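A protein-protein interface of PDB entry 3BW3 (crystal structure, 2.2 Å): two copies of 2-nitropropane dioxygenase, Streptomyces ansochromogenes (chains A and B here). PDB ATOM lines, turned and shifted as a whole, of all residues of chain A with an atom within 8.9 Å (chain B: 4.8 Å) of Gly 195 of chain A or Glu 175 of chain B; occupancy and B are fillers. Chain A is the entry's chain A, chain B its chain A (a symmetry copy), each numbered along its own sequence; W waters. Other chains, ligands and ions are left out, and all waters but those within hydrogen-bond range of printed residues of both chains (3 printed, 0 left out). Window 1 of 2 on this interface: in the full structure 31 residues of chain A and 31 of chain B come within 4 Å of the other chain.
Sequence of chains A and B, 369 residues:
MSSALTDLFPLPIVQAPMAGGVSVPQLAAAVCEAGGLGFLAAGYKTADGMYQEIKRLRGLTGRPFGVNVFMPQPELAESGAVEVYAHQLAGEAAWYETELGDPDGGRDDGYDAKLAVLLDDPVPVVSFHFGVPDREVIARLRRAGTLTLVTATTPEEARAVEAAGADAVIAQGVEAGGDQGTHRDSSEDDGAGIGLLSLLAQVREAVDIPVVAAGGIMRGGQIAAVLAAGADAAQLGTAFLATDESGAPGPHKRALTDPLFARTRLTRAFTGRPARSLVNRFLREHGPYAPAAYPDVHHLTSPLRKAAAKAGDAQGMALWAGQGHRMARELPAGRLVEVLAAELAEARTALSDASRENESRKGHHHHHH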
ATOM      1  N   THR A 153      24.710  35.501  10.515  1.00  0.00           N
ATOM      2  CA  THR A 153      24.295  34.107  10.636  1.00  0.00           C
ATOM      3  C   THR A 153      23.879  33.500   9.293  1.00  0.00           C
ATOM      4  O   THR A 153      23.583  32.303   9.199  1.00  0.00           O
ATOM      5  CB  THR A 153      23.120  33.978  11.626  1.00  0.00           C
ATOM      6  OG1 THR A 153      21.977  34.663  11.103  1.00  0.00           O
ATOM      7  CG2 THR A 153      23.496  34.587  12.976  1.00  0.00           C
ATOM      8  N   ALA A 171      31.076  34.716  11.390  1.00  0.00           N
ATOM      9  CA  ALA A 171      30.086  33.760  10.909  1.00  0.00           C
ATOM     10  C   ALA A 171      29.746  32.821  12.062  1.00  0.00           C
ATOM     11  O   ALA A 171      30.523  31.931  12.397  1.00  0.00           O
ATOM     12  CB  ALA A 171      30.649  32.970   9.732  1.00  0.00           C
ATOM     13  N   GLN A 172      28.585  33.029  12.669  1.00  0.00           N
ATOM     14  CA  GLN A 172      28.142  32.216  13.793  1.00  0.00           C
ATOM     15  C   GLN A 172      27.125  31.164  13.344  1.00  0.00           C
ATOM     16  O   GLN A 172      26.025  31.507  12.910  1.00  0.00           O
ATOM     17  CB  GLN A 172      27.523  33.121  14.861  1.00  0.00           C
ATOM     18  CG  GLN A 172      26.968  32.392  16.077  1.00  0.00           C
ATOM     19  CD  GLN A 172      26.045  33.283  16.888  1.00  0.00           C
ATOM     20  OE1 GLN A 172      25.169  33.947  16.327  1.00  0.00           O
ATOM     21  NE2 GLN A 172      26.228  33.301  18.210  1.00  0.00           N
ATOM     22  N   GLY A 173      27.498  29.888  13.454  1.00  0.00           N
ATOM     23  CA  GLY A 173      26.607  28.808  13.051  1.00  0.00           C
ATOM     24  C   GLY A 173      25.600  28.452  14.129  1.00  0.00           C
ATOM     25  O   GLY A 173      25.666  28.973  15.241  1.00  0.00           O
ATOM     26  N   VAL A 174      24.669  27.553  13.820  1.00  0.00           N
ATOM     27  CA  VAL A 174      23.652  27.174  14.796  1.00  0.00           C
ATOM     28  C   VAL A 174      24.172  26.438  16.011  1.00  0.00           C
ATOM     29  O   VAL A 174      23.495  26.390  17.031  1.00  0.00           O
ATOM     30  CB  VAL A 174      22.558  26.293  14.180  1.00  0.00           C
ATOM     31  CG1 VAL A 174      21.672  27.133  13.345  1.00  0.00           C
ATOM     32  CG2 VAL A 174      23.173  25.165  13.371  1.00  0.00           C
ATOM     33  N   GLU A 175      25.359  25.856  15.899  1.00  0.00           N
ATOM     34  CA  GLU A 175      25.941  25.113  17.010  1.00  0.00           C
ATOM     35  C   GLU A 175      26.374  26.019  18.156  1.00  0.00           C
ATOM     36  O   GLU A 175      26.559  25.554  19.282  1.00  0.00           O
ATOM     37  CB  GLU A 175      27.160  24.313  16.545  1.00  0.00           C
ATOM     38  CG  GLU A 175      26.908  23.408  15.356  1.00  0.00           C
ATOM     39  CD  GLU A 175      27.407  24.019  14.069  1.00  0.00           C
ATOM     40  OE1 GLU A 175      26.952  25.130  13.723  1.00  0.00           O
ATOM     41  OE2 GLU A 175      28.258  23.393  13.412  1.00  0.00           O
ATOM     42  N   ALA A 176      26.535  27.305  17.858  1.00  0.00           N
ATOM     43  CA  ALA A 176      26.989  28.287  18.837  1.00  0.00           C
ATOM     44  C   ALA A 176      26.189  28.329  20.136  1.00  0.00           C
ATOM     45  O   ALA A 176      24.976  28.118  20.143  1.00  0.00           O
ATOM     46  CB  ALA A 176      27.007  29.680  18.197  1.00  0.00           C
ATOM     47  N   GLN A 180      22.036  33.996  19.454  1.00  0.00           N
ATOM     48  CA  GLN A 180      22.267  33.954  18.015  1.00  0.00           C
ATOM     49  C   GLN A 180      22.346  35.434  17.658  1.00  0.00           C
ATOM     50  O   GLN A 180      21.537  36.227  18.141  1.00  0.00           O
ATOM     51  CB  GLN A 180      21.091  33.305  17.281  1.00  0.00           C
ATOM     52  CG  GLN A 180      21.129  31.784  17.246  1.00  0.00           C
ATOM     53  CD  GLN A 180      22.199  31.244  16.312  1.00  0.00           C
ATOM     54  OE1 GLN A 180      23.149  30.593  16.748  1.00  0.00           O
ATOM     55  NE2 GLN A 180      22.050  31.510  15.022  1.00  0.00           N
ATOM     56  N   ALA A 192      15.561  26.960  10.720  1.00  0.00           N
ATOM     57  CA  ALA A 192      16.364  27.228   9.534  1.00  0.00           C
ATOM     58  C   ALA A 192      17.794  27.673   9.866  1.00  0.00           C
ATOM     59  O   ALA A 192      18.402  28.414   9.111  1.00  0.00           O
ATOM     60  CB  ALA A 192      15.670  28.286   8.670  1.00  0.00           C
ATOM     61  N   GLY A 193      18.344  27.244  10.993  1.00  0.00           N
ATOM     62  CA  GLY A 193      19.703  27.654  11.302  1.00  0.00           C
ATOM     63  C   GLY A 193      20.742  26.917  10.466  1.00  0.00           C
ATOM     64  O   GLY A 193      20.600  25.726  10.196  1.00  0.00           O
ATOM     65  N   ILE A 194      21.805  27.613  10.081  1.00  0.00           N
ATOM     66  CA  ILE A 194      22.854  27.020   9.248  1.00  0.00           C
ATOM     67  C   ILE A 194      24.065  26.479  10.019  1.00  0.00           C
ATOM     68  O   ILE A 194      24.621  27.160  10.883  1.00  0.00           O
ATOM     69  CB  ILE A 194      23.353  28.049   8.207  1.00  0.00           C
ATOM     70  CG1 ILE A 194      22.156  28.629   7.442  1.00  0.00           C
ATOM     71  CG2 ILE A 194      24.328  27.393   7.242  1.00  0.00           C
ATOM     72  CD1 ILE A 194      22.521  29.724   6.467  1.00  0.00           C
ATOM     73  N   GLY A 195      24.467  25.250   9.698  1.00  0.00           N
ATOM     74  CA  GLY A 195      25.624  24.655  10.346  1.00  0.00           C
ATOM     75  C   GLY A 195      26.858  25.476  10.011  1.00  0.00           C
ATOM     76  O   GLY A 195      27.000  25.944   8.879  1.00  0.00           O
ATOM     77  N   LEU A 196      27.751  25.650  10.982  1.00  0.00           N
ATOM     78  CA  LEU A 196      28.958  26.453  10.772  1.00  0.00           C
ATOM     79  C   LEU A 196      29.786  26.115   9.540  1.00  0.00           C
ATOM     80  O   LEU A 196      30.193  27.014   8.807  1.00  0.00           O
ATOM     81  CB  LEU A 196      29.876  26.393  12.001  1.00  0.00           C
ATOM     82  CG  LEU A 196      31.164  27.220  11.893  1.00  0.00           C
ATOM     83  CD1 LEU A 196      30.817  28.691  11.676  1.00  0.00           C
ATOM     84  CD2 LEU A 196      31.995  27.059  13.171  1.00  0.00           C
ATOM     85  N   LEU A 197      30.055  24.832   9.312  1.00  0.00           N
ATOM     86  CA  LEU A 197      30.874  24.440   8.168  1.00  0.00           C
ATOM     87  C   LEU A 197      30.246  24.901   6.854  1.00  0.00           C
ATOM     88  O   LEU A 197      30.943  25.262   5.899  1.00  0.00           O
ATOM     89  CB  LEU A 197      31.076  22.923   8.153  1.00  0.00           C
ATOM     90  CG  LEU A 197      32.002  22.372   7.064  1.00  0.00           C
ATOM     91  CD1 LEU A 197      33.398  22.988   7.202  1.00  0.00           C
ATOM     92  CD2 LEU A 197      32.077  20.855   7.184  1.00  0.00           C
ATOM     93  N   SER A 198      28.922  24.896   6.814  1.00  0.00           N
ATOM     94  CA  SER A 198      28.210  25.320   5.622  1.00  0.00           C
ATOM     95  C   SER A 198      28.161  26.847   5.578  1.00  0.00           C
ATOM     96  O   SER A 198      28.425  27.455   4.540  1.00  0.00           O
ATOM     97  CB  SER A 198      26.798  24.736   5.626  1.00  0.00           C
ATOM     98  OG  SER A 198      26.195  24.897   4.359  1.00  0.00           O
ATOM     99  N   LEU A 199      27.841  27.469   6.710  1.00  0.00           N
ATOM    100  CA  LEU A 199      27.774  28.925   6.778  1.00  0.00           C
ATOM    101  C   LEU A 199      29.110  29.563   6.424  1.00  0.00           C
ATOM    102  O   LEU A 199      29.155  30.562   5.707  1.00  0.00           O
ATOM    103  CB  LEU A 199      27.348  29.393   8.173  1.00  0.00           C
ATOM    104  CG  LEU A 199      27.348  30.916   8.372  1.00  0.00           C
ATOM    105  CD1 LEU A 199      26.390  31.562   7.379  1.00  0.00           C
ATOM    106  CD2 LEU A 199      26.947  31.258   9.801  1.00  0.00           C
ATOM    107  N   LEU A 200      30.197  28.990   6.934  1.00  0.00           N
ATOM    108  CA  LEU A 200      31.523  29.524   6.651  1.00  0.00           C
ATOM    109  C   LEU A 200      31.803  29.578   5.150  1.00  0.00           C
ATOM    110  O   LEU A 200      32.270  30.593   4.640  1.00  0.00           O
ATOM    111  CB  LEU A 200      32.595  28.680   7.337  1.00  0.00           C
ATOM    112  CG  LEU A 200      34.044  29.083   7.048  1.00  0.00           C
ATOM    113  CD1 LEU A 200      34.267  30.555   7.387  1.00  0.00           C
ATOM    114  CD2 LEU A 200      34.976  28.201   7.865  1.00  0.00           C
ATOM    115  N   ALA A 201      31.517  28.482   4.450  1.00  0.00           N
ATOM    116  CA  ALA A 201      31.744  28.409   3.010  1.00  0.00           C
ATOM    117  C   ALA A 201      30.877  29.414   2.262  1.00  0.00           C
ATOM    118  O   ALA A 201      31.345  30.065   1.327  1.00  0.00           O
ATOM    119  CB  ALA A 201      31.464  26.997   2.506  1.00  0.00           C
ATOM    120  N   GLN A 202      29.616  29.539   2.677  1.00  0.00           N
ATOM    121  CA  GLN A 202      28.689  30.478   2.049  1.00  0.00           C
ATOM    122  C   GLN A 202      29.150  31.918   2.245  1.00  0.00           C
ATOM    123  O   GLN A 202      29.133  32.724   1.315  1.00  0.00           O
ATOM    124  CB  GLN A 202      27.281  30.322   2.635  1.00  0.00           C
ATOM    125  CG  GLN A 202      26.579  29.007   2.286  1.00  0.00           C
ATOM    126  CD  GLN A 202      25.187  28.929   2.886  1.00  0.00           C
ATOM    127  OE1 GLN A 202      24.373  29.829   2.706  1.00  0.00           O
ATOM    128  NE2 GLN A 202      24.908  27.851   3.600  1.00  0.00           N
ATOM    129  N   VAL A 203      29.555  32.236   3.469  1.00  0.00           N
ATOM    130  CA  VAL A 203      30.016  33.573   3.790  1.00  0.00           C
ATOM    131  C   VAL A 203      31.327  33.904   3.080  1.00  0.00           C
ATOM    132  O   VAL A 203      31.518  35.025   2.609  1.00  0.00           O
ATOM    133  CB  VAL A 203      30.195  33.739   5.310  1.00  0.00           C
ATOM    134  CG1 VAL A 203      30.904  35.045   5.609  1.00  0.00           C
ATOM    135  CG2 VAL A 203      28.828  33.710   5.996  1.00  0.00           C
ATOM    136  N   ALA A 214      32.567  30.931  14.268  1.00  0.00           N
ATOM    137  CA  ALA A 214      32.079  30.709  15.629  1.00  0.00           C
ATOM    138  C   ALA A 214      30.968  29.664  15.717  1.00  0.00           C
ATOM    139  O   ALA A 214      30.021  29.678  14.928  1.00  0.00           O
ATOM    140  CB  ALA A 214      31.582  32.030  16.232  1.00  0.00           C
ATOM    141  N   GLY A 215      31.080  28.773  16.697  1.00  0.00           N
ATOM    142  CA  GLY A 215      30.065  27.750  16.878  1.00  0.00           C
ATOM    143  C   GLY A 215      30.577  26.337  17.093  1.00  0.00           C
ATOM    144  O   GLY A 215      31.043  25.685  16.162  1.00  0.00           O
ATOM    145  N   ARG A 276      21.089  29.400  22.330  1.00  0.00           N
ATOM    146  CA  ARG A 276      21.292  28.001  22.697  1.00  0.00           C
ATOM    147  C   ARG A 276      21.671  27.785  24.162  1.00  0.00           C
ATOM    148  O   ARG A 276      22.660  28.335  24.662  1.00  0.00           O
ATOM    149  CB  ARG A 276      22.346  27.369  21.783  1.00  0.00           C
ATOM    150  CG  ARG A 276      22.521  25.867  21.998  1.00  0.00           C
ATOM    151  CD  ARG A 276      23.478  25.258  20.985  1.00  0.00           C
ATOM    152  NE  ARG A 276      22.947  25.303  19.626  1.00  0.00           N
ATOM    153  CZ  ARG A 276      22.008  24.483  19.149  1.00  0.00           C
ATOM    154  NH1 ARG A 276      21.485  23.537  19.919  1.00  0.00           N
ATOM    155  NH2 ARG A 276      21.585  24.614  17.896  1.00  0.00           N
ATOM    156  N   GLN A 323      27.011  23.284  21.143  1.00  0.00           N
ATOM    157  CA  GLN A 323      26.861  21.838  21.045  1.00  0.00           C
ATOM    158  C   GLN A 323      28.110  21.043  21.447  1.00  0.00           C
ATOM    159  O   GLN A 323      28.056  19.826  21.583  1.00  0.00           O
ATOM    160  CB  GLN A 323      26.412  21.456  19.629  1.00  0.00           C
ATOM    161  CG  GLN A 323      25.078  22.073  19.211  1.00  0.00           C
ATOM    162  CD  GLN A 323      24.600  21.578  17.857  1.00  0.00           C
ATOM    163  OE1 GLN A 323      25.369  21.520  16.909  1.00  0.00           O
ATOM    164  NE2 GLN A 323      23.323  21.228  17.763  1.00  0.00           N
ATOM    165  N   GLY B 173      25.732  15.334   9.752  1.00  0.00           N
ATOM    166  CA  GLY B 173      25.261  16.491  10.503  1.00  0.00           C
ATOM    167  C   GLY B 173      23.906  16.981  10.027  1.00  0.00           C
ATOM    168  O   GLY B 173      23.379  16.486   9.032  1.00  0.00           O
ATOM    169  N   VAL B 174      23.337  17.965  10.718  1.00  0.00           N
ATOM    170  CA  VAL B 174      22.024  18.475  10.336  1.00  0.00           C
ATOM    171  C   VAL B 174      21.976  19.185   9.000  1.00  0.00           C
ATOM    172  O   VAL B 174      20.904  19.332   8.424  1.00  0.00           O
ATOM    173  CB  VAL B 174      21.457  19.451  11.374  1.00  0.00           C
ATOM    174  CG1 VAL B 174      20.992  18.687  12.552  1.00  0.00           C
ATOM    175  CG2 VAL B 174      22.498  20.484  11.760  1.00  0.00           C
ATOM    176  N   GLU B 175      23.127  19.634   8.517  1.00  0.00           N
ATOM    177  CA  GLU B 175      23.184  20.341   7.244  1.00  0.00           C
ATOM    178  C   GLU B 175      22.919  19.426   6.055  1.00  0.00           C
ATOM    179  O   GLU B 175      22.592  19.899   4.963  1.00  0.00           O
ATOM    180  CB  GLU B 175      24.554  20.995   7.049  1.00  0.00           C
ATOM    181  CG  GLU B 175      24.997  21.889   8.189  1.00  0.00           C
ATOM    182  CD  GLU B 175      25.981  21.194   9.098  1.00  0.00           C
ATOM    183  OE1 GLU B 175      25.632  20.129   9.649  1.00  0.00           O
ATOM    184  OE2 GLU B 175      27.104  21.709   9.253  1.00  0.00           O
ATOM    185  N   ALA B 176      23.065  18.123   6.274  1.00  0.00           N
ATOM    186  CA  ALA B 176      22.890  17.124   5.224  1.00  0.00           C
ATOM    187  C   ALA B 176      21.569  17.202   4.465  1.00  0.00           C
ATOM    188  O   ALA B 176      20.529  17.541   5.031  1.00  0.00           O
ATOM    189  CB  ALA B 176      23.064  15.721   5.815  1.00  0.00           C
ATOM    190  N   GLY B 177      21.624  16.893   3.173  1.00  0.00           N
ATOM    191  CA  GLY B 177      20.422  16.889   2.363  1.00  0.00           C
ATOM    192  C   GLY B 177      19.791  15.509   2.450  1.00  0.00           C
ATOM    193  O   GLY B 177      20.454  14.542   2.818  1.00  0.00           O
ATOM    194  N   ILE B 194      22.614  18.108  15.370  1.00  0.00           N
ATOM    195  CA  ILE B 194      23.989  18.564  15.586  1.00  0.00           C
ATOM    196  C   ILE B 194      24.736  18.993  14.315  1.00  0.00           C
ATOM    197  O   ILE B 194      24.737  18.281  13.311  1.00  0.00           O
ATOM    198  CB  ILE B 194      24.812  17.459  16.290  1.00  0.00           C
ATOM    199  CG1 ILE B 194      24.071  16.989  17.549  1.00  0.00           C
ATOM    200  CG2 ILE B 194      26.193  17.982  16.655  1.00  0.00           C
ATOM    201  CD1 ILE B 194      24.738  15.836  18.261  1.00  0.00           C
ATOM    202  N   GLY B 195      25.370  20.164  14.373  1.00  0.00           N
ATOM    203  CA  GLY B 195      26.134  20.651  13.236  1.00  0.00           C
ATOM    204  C   GLY B 195      27.283  19.694  12.965  1.00  0.00           C
ATOM    205  O   GLY B 195      27.897  19.184  13.904  1.00  0.00           O
ATOM    206  N   LEU B 196      27.581  19.453  11.690  1.00  0.00           N
ATOM    207  CA  LEU B 196      28.649  18.522  11.321  1.00  0.00           C
ATOM    208  C   LEU B 196      29.995  18.737  11.998  1.00  0.00           C
ATOM    209  O   LEU B 196      30.604  17.780  12.473  1.00  0.00           O
ATOM    210  CB  LEU B 196      28.870  18.517   9.801  1.00  0.00           C
ATOM    211  CG  LEU B 196      29.958  17.555   9.305  1.00  0.00           C
ATOM    212  CD1 LEU B 196      29.603  16.125   9.700  1.00  0.00           C
ATOM    213  CD2 LEU B 196      30.091  17.661   7.781  1.00  0.00           C
ATOM    214  N   LEU B 197      30.474  19.977  12.037  1.00  0.00           N
ATOM    215  CA  LEU B 197      31.776  20.249  12.641  1.00  0.00           C
ATOM    216  C   LEU B 197      31.806  19.821  14.107  1.00  0.00           C
ATOM    217  O   LEU B 197      32.831  19.363  14.623  1.00  0.00           O
ATOM    218  CB  LEU B 197      32.120  21.735  12.517  1.00  0.00           C
ATOM    219  CG  LEU B 197      33.505  22.156  13.016  1.00  0.00           C
ATOM    220  CD1 LEU B 197      34.593  21.398  12.247  1.00  0.00           C
ATOM    221  CD2 LEU B 197      33.675  23.659  12.835  1.00  0.00           C
ATOM    222  N   GLY B 215      27.430  16.150   5.166  1.00  0.00           N
ATOM    223  CA  GLY B 215      26.566  17.279   5.463  1.00  0.00           C
ATOM    224  C   GLY B 215      27.060  18.636   4.992  1.00  0.00           C
ATOM    225  O   GLY B 215      27.980  19.209   5.570  1.00  0.00           O
ATOM    226  N   GLY B 216      26.445  19.141   3.928  1.00  0.00           N
ATOM    227  CA  GLY B 216      26.793  20.447   3.395  1.00  0.00           C
ATOM    228  C   GLY B 216      28.150  20.626   2.742  1.00  0.00           C
ATOM    229  O   GLY B 216      28.573  21.764   2.538  1.00  0.00           O
ATOM    230  N   ARG B 276      15.959  16.738   4.998  1.00  0.00           N
ATOM    231  CA  ARG B 276      16.109  18.117   4.542  1.00  0.00           C
ATOM    232  C   ARG B 276      15.764  18.330   3.068  1.00  0.00           C
ATOM    233  O   ARG B 276      16.331  17.692   2.171  1.00  0.00           O
ATOM    234  CB  ARG B 276      17.531  18.609   4.823  1.00  0.00           C
ATOM    235  CG  ARG B 276      17.741  20.089   4.511  1.00  0.00           C
ATOM    236  CD  ARG B 276      19.124  20.565   4.929  1.00  0.00           C
ATOM    237  NE  ARG B 276      19.304  20.541   6.378  1.00  0.00           N
ATOM    238  CZ  ARG B 276      18.799  21.442   7.222  1.00  0.00           C
ATOM    239  NH1 ARG B 276      18.075  22.459   6.770  1.00  0.00           N
ATOM    240  NH2 ARG B 276      19.013  21.322   8.529  1.00  0.00           N
ATOM    241  N   GLY B 322      21.061  19.659   0.746  1.00  0.00           N
ATOM    242  CA  GLY B 322      21.780  20.067   1.938  1.00  0.00           C
ATOM    243  C   GLY B 322      21.849  21.582   1.959  1.00  0.00           C
ATOM    244  O   GLY B 322      21.471  22.230   0.981  1.00  0.00           O
ATOM    245  N   GLN B 323      22.340  22.157   3.053  1.00  0.00           N
ATOM    246  CA  GLN B 323      22.410  23.608   3.171  1.00  0.00           C
ATOM    247  C   GLN B 323      23.392  24.277   2.200  1.00  0.00           C
ATOM    248  O   GLN B 323      23.408  25.496   2.074  1.00  0.00           O
ATOM    249  CB  GLN B 323      22.733  23.997   4.619  1.00  0.00           C
ATOM    250  CG  GLN B 323      21.703  23.514   5.638  1.00  0.00           C
ATOM    251  CD  GLN B 323      21.984  24.020   7.042  1.00  0.00           C
ATOM    252  OE1 GLN B 323      23.113  23.971   7.506  1.00  0.00           O
ATOM    253  NE2 GLN B 323      20.952  24.500   7.725  1.00  0.00           N
HETATM  254  O   HOH W   1      28.270  21.685   6.696  1.00  0.00           O
HETATM  255  O   HOH W   2      17.819  24.150   9.083  1.00  0.00           O
HETATM  256  O   HOH W   3      27.840  24.236   2.449  1.00  0.00           O
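The side-chain amide nitrogen of Gln 202 of chain A is in hydrogen-bond range of the backbone carbonyl oxygen of Gln 323 of chain B (3.2 Å).
OE1 of Gln 323 of chain A is in hydrogen-bond range of N of Gly 195 of chain B (2.9 Å).
The backbone NH (N) of Gly 195 of chain A lies within hydrogen-bond range of the side-chain amide oxygen (OE1) of Gln 323 of chain B (2.9 Å).
The backbone carbonyl oxygen (O) of Gly 193 of chain A is in hydrogen-bond range of the side-chain amide nitrogen (NE2) of Gln 323 of chain B.
N of Gln 323 of chain A is in hydrogen-bond range of O of Glu 175 of chain A (3.0 Å).
N of Val 174 of chain A is in hydrogen-bond range of O of Ile 194 of chain A (3.0 Å).
The side-chain carboxylate (OE1) of Glu 175 of chain B is in hydrogen-bond range of the backbone NH (N) of Leu 196 of chain B (2.9 Å).
OG of Ser 198 of chain A is in hydrogen-bond range of NE2 of Gln 202 of chain A, at 3.3 Å.
OE1 of Glu 175 of chain A is in hydrogen-bond range of N of Leu 196 of chain A (2.9 Å).
The backbone NH of Val 174 of chain B lies within hydrogen-bond range of the backbone carbonyl oxygen of Ile 194 of chain B, 3.0 Å away.
OE2 of Glu 175 of chain A touches CA of Gly 195 of chain B, 3.5 Å away.
NE2 of Gln 323 of chain B touches CA of Ile 194 of chain A (3.5 Å).
CA of Gly 195 of chain A touches OE2 of Glu 175 of chain B, at 3.5 Å.
Leu 196 of chain A touches Leu 197 of chain B (CD2 to CD2, 3.8 Å).
Leu 197 of chain A touches Leu 196 of chain B (CD2 to CD2, 3.8 Å).
OG of Ser 198 of chain A touches CB of Gln 323 of chain B, 3.6 Å away.
Gln 323 of chain A touches Ile 194 of chain B (NE2 to CA, 3.5 Å).
Gly 195 of chain A touches just these residues of chain B: Glu 175 (3.5 Å) and Gln 323 (2.9 Å).
No residue of chain A comes within 4 Å of Gly 173 of chain B.
No residue of chain A comes within 4 Å of Val 174 of chain B.
No residue of chain A comes within 4 Å of Ala 176 of chain B.
No residue of chain A comes within 4 Å of Gly 322 of chain B.
Printed residues of chain B within 4 Å of Ile 194 of chain A: Gln 323 (3.5 Å).
Printed residues of chain A within 4 Å of Ile 194 of chain B: Gln 323.
Of the printed residues of chain B, Gly 193 of chain A touches Gln 323.
Val 203 of chain A touches none of the printed residues of chain B.
Leu 200 of chain A touches none of the printed residues of chain B.
Hydrophobic or aromatic side chains of chain B that line the printed part of chain A: Ile 194, Leu 196 and Leu 197.
Along chain B the printed residues that touch a printed residue of chain A span positions 175 to 323.
Printed residues of chain A that touch a printed residue of chain B: Glu 175, Gly 193, Ile 194, Gly 195, Leu 196, Leu 197, Ser 198, Gln 202 and Gln 323.
Hydrophobic or aromatic side chains of chain A within 4 Å of the printed part of chain B: Ile 194, Leu 196 and Leu 197.
Along chain A the printed residues that touch a printed residue of chain B span positions 175 to 323.
Among the printed residues, no Asp or Glu carboxylate lies within 4 Å of a Lys or Arg side-chain nitrogen of the other chain.
Glu 175 of chain A touches Gly 195 of chain B, and with the chains exchanged Gly 195 of chain A touches Glu 175 of chain B.
Ile 194 of chain A touches Gln 323 of chain B, and with the chains exchanged Gln 323 of chain A touches Ile 194 of chain B.
Gly 195 of chain A touches Gln 323 of chain B, and with the chains exchanged Gln 323 of chain A touches Gly 195 of chain B.
Leu 196 of chain A touches Leu 197 of chain B, and with the chains exchanged Leu 197 of chain A touches Leu 196 of chain B.
Positions printed for both chains: 173, 174, 175, 176, 194, 195, 196, 197, 215, 276 and 323.
Water W3 lies within hydrogen-bond range of the backbone carbonyl oxygen (O) of Gly 216 of chain B and the side-chain hydroxyl (OG) of Ser 198 of chain A.
Water W1 lies within hydrogen-bond range of O of Gly 215 of chain B (2.7 Å), OE2 of Glu 175 of chain B (2.8 Å) and N of Ser 198 of chain A (3.3 Å).
Water W2 lies within hydrogen-bond range of NH1 of Arg 276 of chain B (2.9 Å), O of Gly 193 of chain A (3.4 Å) and NE2 of Gln 323 of chain B (3.4 Å).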
